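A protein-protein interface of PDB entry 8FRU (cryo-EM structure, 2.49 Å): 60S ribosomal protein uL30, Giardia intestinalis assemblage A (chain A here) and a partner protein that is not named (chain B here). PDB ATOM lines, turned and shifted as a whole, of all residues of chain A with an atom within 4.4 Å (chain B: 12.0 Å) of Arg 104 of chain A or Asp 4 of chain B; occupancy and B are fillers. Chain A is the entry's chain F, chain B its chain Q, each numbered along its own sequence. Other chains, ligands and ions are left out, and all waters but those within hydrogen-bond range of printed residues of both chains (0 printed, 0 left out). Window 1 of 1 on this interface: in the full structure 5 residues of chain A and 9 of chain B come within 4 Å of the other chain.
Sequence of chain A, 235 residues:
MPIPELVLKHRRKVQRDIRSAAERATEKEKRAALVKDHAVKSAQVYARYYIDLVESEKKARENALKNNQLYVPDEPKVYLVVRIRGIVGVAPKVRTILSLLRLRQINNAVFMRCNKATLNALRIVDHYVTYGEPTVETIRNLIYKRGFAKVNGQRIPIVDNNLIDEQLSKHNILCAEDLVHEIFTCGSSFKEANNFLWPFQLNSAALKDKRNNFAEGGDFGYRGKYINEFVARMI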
ATOM      1  N   ARG A  83      23.604 -18.935  12.578  1.00  0.00           N
ATOM      2  CA  ARG A  83      22.771 -17.893  13.166  1.00  0.00           C
ATOM      3  C   ARG A  83      21.607 -18.514  13.932  1.00  0.00           C
ATOM      4  O   ARG A  83      20.901 -19.377  13.410  1.00  0.00           O
ATOM      5  CB  ARG A  83      22.253 -16.954  12.078  1.00  0.00           C
ATOM      6  CG  ARG A  83      21.676 -15.654  12.594  1.00  0.00           C
ATOM      7  CD  ARG A  83      20.968 -14.879  11.506  1.00  0.00           C
ATOM      8  NE  ARG A  83      20.192 -13.776  12.054  1.00  0.00           N
ATOM      9  CZ  ARG A  83      20.100 -12.574  11.505  1.00  0.00           C
ATOM     10  NH1 ARG A  83      20.714 -12.281  10.374  1.00  0.00           N
ATOM     11  NH2 ARG A  83      19.382 -11.638  12.116  1.00  0.00           N
ATOM     12  N   ILE A  87      15.320 -11.672  13.082  1.00  0.00           N
ATOM     13  CA  ILE A  87      15.583 -10.450  12.334  1.00  0.00           C
ATOM     14  C   ILE A  87      14.794  -9.254  12.849  1.00  0.00           C
ATOM     15  O   ILE A  87      14.745  -8.227  12.182  1.00  0.00           O
ATOM     16  CB  ILE A  87      15.323 -10.651  10.827  1.00  0.00           C
ATOM     17  CG1 ILE A  87      13.890 -11.114  10.586  1.00  0.00           C
ATOM     18  CG2 ILE A  87      16.302 -11.640  10.233  1.00  0.00           C
ATOM     19  CD1 ILE A  87      13.177 -10.348   9.517  1.00  0.00           C
ATOM     20  N   SER A  99      25.349  -9.148   7.696  1.00  0.00           N
ATOM     21  CA  SER A  99      25.244  -9.131   6.242  1.00  0.00           C
ATOM     22  C   SER A  99      26.559  -9.522   5.583  1.00  0.00           C
ATOM     23  O   SER A  99      26.565 -10.228   4.570  1.00  0.00           O
ATOM     24  CB  SER A  99      24.796  -7.752   5.770  1.00  0.00           C
ATOM     25  OG  SER A  99      25.381  -7.429   4.528  1.00  0.00           O
ATOM     26  N   ARG A 102      27.116 -13.242   5.330  1.00  0.00           N
ATOM     27  CA  ARG A 102      26.096 -13.955   4.569  1.00  0.00           C
ATOM     28  C   ARG A 102      25.164 -14.766   5.463  1.00  0.00           C
ATOM     29  O   ARG A 102      24.676 -15.820   5.063  1.00  0.00           O
ATOM     30  CB  ARG A 102      26.717 -14.856   3.499  1.00  0.00           C
ATOM     31  CG  ARG A 102      27.713 -14.158   2.613  1.00  0.00           C
ATOM     32  CD  ARG A 102      28.778 -15.109   2.120  1.00  0.00           C
ATOM     33  NE  ARG A 102      28.406 -15.726   0.855  1.00  0.00           N
ATOM     34  CZ  ARG A 102      28.569 -17.009   0.566  1.00  0.00           C
ATOM     35  NH1 ARG A 102      29.112 -17.849   1.429  1.00  0.00           N
ATOM     36  NH2 ARG A 102      28.176 -17.460  -0.618  1.00  0.00           N
ATOM     37  N   LEU A 103      24.883 -14.279   6.667  1.00  0.00           N
ATOM     38  CA  LEU A 103      23.959 -14.937   7.588  1.00  0.00           C
ATOM     39  C   LEU A 103      22.723 -14.052   7.726  1.00  0.00           C
ATOM     40  O   LEU A 103      22.586 -13.284   8.675  1.00  0.00           O
ATOM     41  CB  LEU A 103      24.624 -15.183   8.929  1.00  0.00           C
ATOM     42  CG  LEU A 103      25.684 -16.280   8.980  1.00  0.00           C
ATOM     43  CD1 LEU A 103      26.268 -16.383  10.362  1.00  0.00           C
ATOM     44  CD2 LEU A 103      25.095 -17.598   8.553  1.00  0.00           C
ATOM     45  N   ARG A 104      21.814 -14.170   6.764  1.00  0.00           N
ATOM     46  CA  ARG A 104      20.658 -13.291   6.665  1.00  0.00           C
ATOM     47  C   ARG A 104      19.369 -13.913   7.180  1.00  0.00           C
ATOM     48  O   ARG A 104      18.332 -13.248   7.160  1.00  0.00           O
ATOM     49  CB  ARG A 104      20.469 -12.847   5.213  1.00  0.00           C
ATOM     50  CG  ARG A 104      21.697 -12.192   4.614  1.00  0.00           C
ATOM     51  CD  ARG A 104      21.410 -11.601   3.250  1.00  0.00           C
ATOM     52  NE  ARG A 104      21.331 -10.147   3.304  1.00  0.00           N
ATOM     53  CZ  ARG A 104      22.186  -9.327   2.714  1.00  0.00           C
ATOM     54  NH1 ARG A 104      23.197  -9.784   1.998  1.00  0.00           N
ATOM     55  NH2 ARG A 104      22.021  -8.016   2.845  1.00  0.00           N
ATOM     56  N   GLN A 105      19.404 -15.156   7.648  1.00  0.00           N
ATOM     57  CA  GLN A 105      18.199 -15.845   8.080  1.00  0.00           C
ATOM     58  C   GLN A 105      18.548 -16.749   9.250  1.00  0.00           C
ATOM     59  O   GLN A 105      19.693 -17.165   9.416  1.00  0.00           O
ATOM     60  CB  GLN A 105      17.575 -16.643   6.928  1.00  0.00           C
ATOM     61  CG  GLN A 105      16.239 -17.257   7.245  1.00  0.00           C
ATOM     62  CD  GLN A 105      15.672 -18.076   6.107  1.00  0.00           C
ATOM     63  OE1 GLN A 105      16.372 -18.863   5.480  1.00  0.00           O
ATOM     64  NE2 GLN A 105      14.392 -17.899   5.844  1.00  0.00           N
ATOM     65  N   MET B   1       9.683 -16.144   3.526  1.00  0.00           N
ATOM     66  CA  MET B   1       9.464 -15.345   4.725  1.00  0.00           C
ATOM     67  C   MET B   1      10.726 -15.246   5.588  1.00  0.00           C
ATOM     68  O   MET B   1      11.716 -15.926   5.325  1.00  0.00           O
ATOM     69  CB  MET B   1       8.314 -15.932   5.549  1.00  0.00           C
ATOM     70  CG  MET B   1       7.177 -16.506   4.723  1.00  0.00           C
ATOM     71  SD  MET B   1       6.048 -17.554   5.669  1.00  0.00           S
ATOM     72  CE  MET B   1       6.247 -19.141   4.862  1.00  0.00           C
ATOM     73  N   GLY B   2      10.677 -14.372   6.593  1.00  0.00           N
ATOM     74  CA  GLY B   2      11.665 -14.316   7.668  1.00  0.00           C
ATOM     75  C   GLY B   2      13.103 -14.101   7.251  1.00  0.00           C
ATOM     76  O   GLY B   2      14.001 -14.761   7.784  1.00  0.00           O
ATOM     77  N   ILE B   3      13.353 -13.179   6.325  1.00  0.00           N
ATOM     78  CA  ILE B   3      14.695 -12.951   5.801  1.00  0.00           C
ATOM     79  C   ILE B   3      14.966 -11.455   5.734  1.00  0.00           C
ATOM     80  O   ILE B   3      14.048 -10.644   5.587  1.00  0.00           O
ATOM     81  CB  ILE B   3      14.880 -13.602   4.412  1.00  0.00           C
ATOM     82  CG1 ILE B   3      16.317 -13.426   3.921  1.00  0.00           C
ATOM     83  CG2 ILE B   3      13.901 -13.022   3.411  1.00  0.00           C
ATOM     84  CD1 ILE B   3      16.882 -14.650   3.265  1.00  0.00           C
ATOM     85  N   ASP B   4      16.240 -11.089   5.842  1.00  0.00           N
ATOM     86  CA  ASP B   4      16.670  -9.698   5.760  1.00  0.00           C
ATOM     87  C   ASP B   4      17.200  -9.413   4.362  1.00  0.00           C
ATOM     88  O   ASP B   4      18.198 -10.004   3.941  1.00  0.00           O
ATOM     89  CB  ASP B   4      17.741  -9.386   6.801  1.00  0.00           C
ATOM     90  CG  ASP B   4      17.702  -7.941   7.252  1.00  0.00           C
ATOM     91  OD1 ASP B   4      16.709  -7.551   7.901  1.00  0.00           O
ATOM     92  OD2 ASP B   4      18.654  -7.188   6.950  1.00  0.00           O
ATOM     93  N   LEU B   5      16.549  -8.490   3.654  1.00  0.00           N
ATOM     94  CA  LEU B   5      16.923  -8.180   2.280  1.00  0.00           C
ATOM     95  C   LEU B   5      17.112  -6.686   2.054  1.00  0.00           C
ATOM     96  O   LEU B   5      17.100  -6.237   0.906  1.00  0.00           O
ATOM     97  CB  LEU B   5      15.883  -8.731   1.307  1.00  0.00           C
ATOM     98  CG  LEU B   5      15.988 -10.230   1.042  1.00  0.00           C
ATOM     99  CD1 LEU B   5      14.808 -10.713   0.231  1.00  0.00           C
ATOM    100  CD2 LEU B   5      17.289 -10.554   0.342  1.00  0.00           C
ATOM    101  N   LYS B   6      17.296  -5.910   3.115  1.00  0.00           N
ATOM    102  CA  LYS B   6      17.406  -4.460   3.011  1.00  0.00           C
ATOM    103  C   LYS B   6      18.582  -3.951   3.829  1.00  0.00           C
ATOM    104  O   LYS B   6      18.478  -2.970   4.564  1.00  0.00           O
ATOM    105  CB  LYS B   6      16.112  -3.790   3.460  1.00  0.00           C
ATOM    106  CG  LYS B   6      15.519  -4.395   4.713  1.00  0.00           C
ATOM    107  CD  LYS B   6      14.608  -3.419   5.436  1.00  0.00           C
ATOM    108  CE  LYS B   6      13.309  -3.201   4.684  1.00  0.00           C
ATOM    109  NZ  LYS B   6      12.533  -2.073   5.267  1.00  0.00           N
ATOM    110  N   THR B   7      19.731  -4.610   3.714  1.00  0.00           N
ATOM    111  CA  THR B   7      20.909  -4.186   4.458  1.00  0.00           C
ATOM    112  C   THR B   7      22.060  -3.773   3.557  1.00  0.00           C
ATOM    113  O   THR B   7      22.677  -2.729   3.794  1.00  0.00           O
ATOM    114  CB  THR B   7      21.373  -5.286   5.415  1.00  0.00           C
ATOM    115  OG1 THR B   7      20.329  -5.571   6.352  1.00  0.00           O
ATOM    116  CG2 THR B   7      22.607  -4.827   6.169  1.00  0.00           C
ATOM    117  N   GLY B   8      22.374  -4.554   2.535  1.00  0.00           N
ATOM    118  CA  GLY B   8      23.409  -4.143   1.609  1.00  0.00           C
ATOM    119  C   GLY B   8      22.913  -4.051   0.184  1.00  0.00           C
ATOM    120  O   GLY B   8      23.688  -4.222  -0.758  1.00  0.00           O
ATOM    121  N   ILE B   9      21.624  -3.775   0.011  1.00  0.00           N
ATOM    122  CA  ILE B   9      20.969  -3.864  -1.286  1.00  0.00           C
ATOM    123  C   ILE B   9      20.198  -2.581  -1.557  1.00  0.00           C
ATOM    124  O   ILE B   9      19.619  -1.988  -0.641  1.00  0.00           O
ATOM    125  CB  ILE B   9      20.038  -5.089  -1.349  1.00  0.00           C
ATOM    126  CG1 ILE B   9      20.796  -6.333  -0.892  1.00  0.00           C
ATOM    127  CG2 ILE B   9      19.497  -5.270  -2.747  1.00  0.00           C
ATOM    128  CD1 ILE B   9      19.922  -7.527  -0.652  1.00  0.00           C
ATOM    129  N   LYS B  10      20.193  -2.156  -2.817  1.00  0.00           N
ATOM    130  CA  LYS B  10      19.523  -0.939  -3.248  1.00  0.00           C
ATOM    131  C   LYS B  10      18.263  -1.267  -4.039  1.00  0.00           C
ATOM    132  O   LYS B  10      18.058  -2.395  -4.492  1.00  0.00           O
ATOM    133  CB  LYS B  10      20.456  -0.076  -4.101  1.00  0.00           C
ATOM    134  CG  LYS B  10      21.918  -0.227  -3.752  1.00  0.00           C
ATOM    135  CD  LYS B  10      22.272   0.578  -2.516  1.00  0.00           C
ATOM    136  CE  LYS B  10      23.702   1.069  -2.579  1.00  0.00           C
ATOM    137  NZ  LYS B  10      23.845   2.192  -3.534  1.00  0.00           N
ATOM    138  N   LYS B  11      17.418  -0.254  -4.202  1.00  0.00           N
ATOM    139  CA  LYS B  11      16.175  -0.407  -4.943  1.00  0.00           C
ATOM    140  C   LYS B  11      16.451  -0.635  -6.426  1.00  0.00           C
ATOM    141  O   LYS B  11      17.487  -0.230  -6.957  1.00  0.00           O
ATOM    142  CB  LYS B  11      15.298   0.829  -4.755  1.00  0.00           C
ATOM    143  CG  LYS B  11      13.851   0.656  -5.177  1.00  0.00           C
ATOM    144  CD  LYS B  11      13.236   1.993  -5.582  1.00  0.00           C
ATOM    145  CE  LYS B  11      11.723   1.994  -5.413  1.00  0.00           C
ATOM    146  NZ  LYS B  11      11.067   0.873  -6.136  1.00  0.00           N
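O of Asp 4 of chain B sits at hydrogen-bond distance from NE of Arg 104 of chain A, at 3.2 Å.
O of Met 1 of chain B is in hydrogen-bond range of NE2 of Gln 105 of chain A, at 3.4 Å.
The guanidinium group (NH2) of Arg 104 of chain A lies close to the backbone NH (N) of Gly 8 of chain B (3.5 Å).
No residue of chain B comes within 4 Å of Ile 87 of chain A.
Of chain B, only Thr 7 (3.7 Å) comes within 4 Å of Ser 99 of chain A.
Of the printed residues of chain B, Arg 104 of chain A touches Ile 3 (3.8 Å), Asp 4 (3.2 Å), Thr 7 (3.8 Å) and Gly 8 (3.5 Å).
Printed residues of chain A within 4 Å of Met 1 of chain B: Gln 105.
Printed residues of chain A within 4 Å of Gly 2 of chain B: Gln 105 (3.4 Å).
Asp 4 of chain B touches just one residue of chain A: Arg 104.
Of the printed residues of chain A, Thr 7 of chain B touches Ser 99 and Arg 104.
Of the printed residues of chain A, Gly 8 of chain B touches Arg 104.
Lys 10 of chain B touches none of the printed residues of chain A.
Lys 11 of chain B touches none of the printed residues of chain A.
The nearest residue of chain B that does not touch Arg 104 of chain A is Ile 9 of chain B (4.1 Å).
The nearest printed residue of chain A that does not touch Asp 4 of chain B is Ile 87 of chain A (4.4 Å).
The nearest printed residue of chain A that does not touch Thr 7 of chain B is Arg 83 of chain A (7.8 Å).
Among the printed residues, merely in contact across the chains: Ser 99 of chain A with Thr 7 of chain B (3.7 Å), Arg 104 of chain A with Ile 3 of chain B (3.8 Å), Arg 104 of chain A with Thr 7 of chain B (3.8 Å) and Gln 105 of chain A with Gly 2 of chain B (3.4 Å).
The side-chain carboxylate (OD2) of Asp 4 of chain B lies within hydrogen-bond range of the side-chain hydroxyl (OG1) of Thr 7 of chain B (2.4 Å).
Of the 11 printed residues of chain B, 6 touch a printed residue of chain A.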
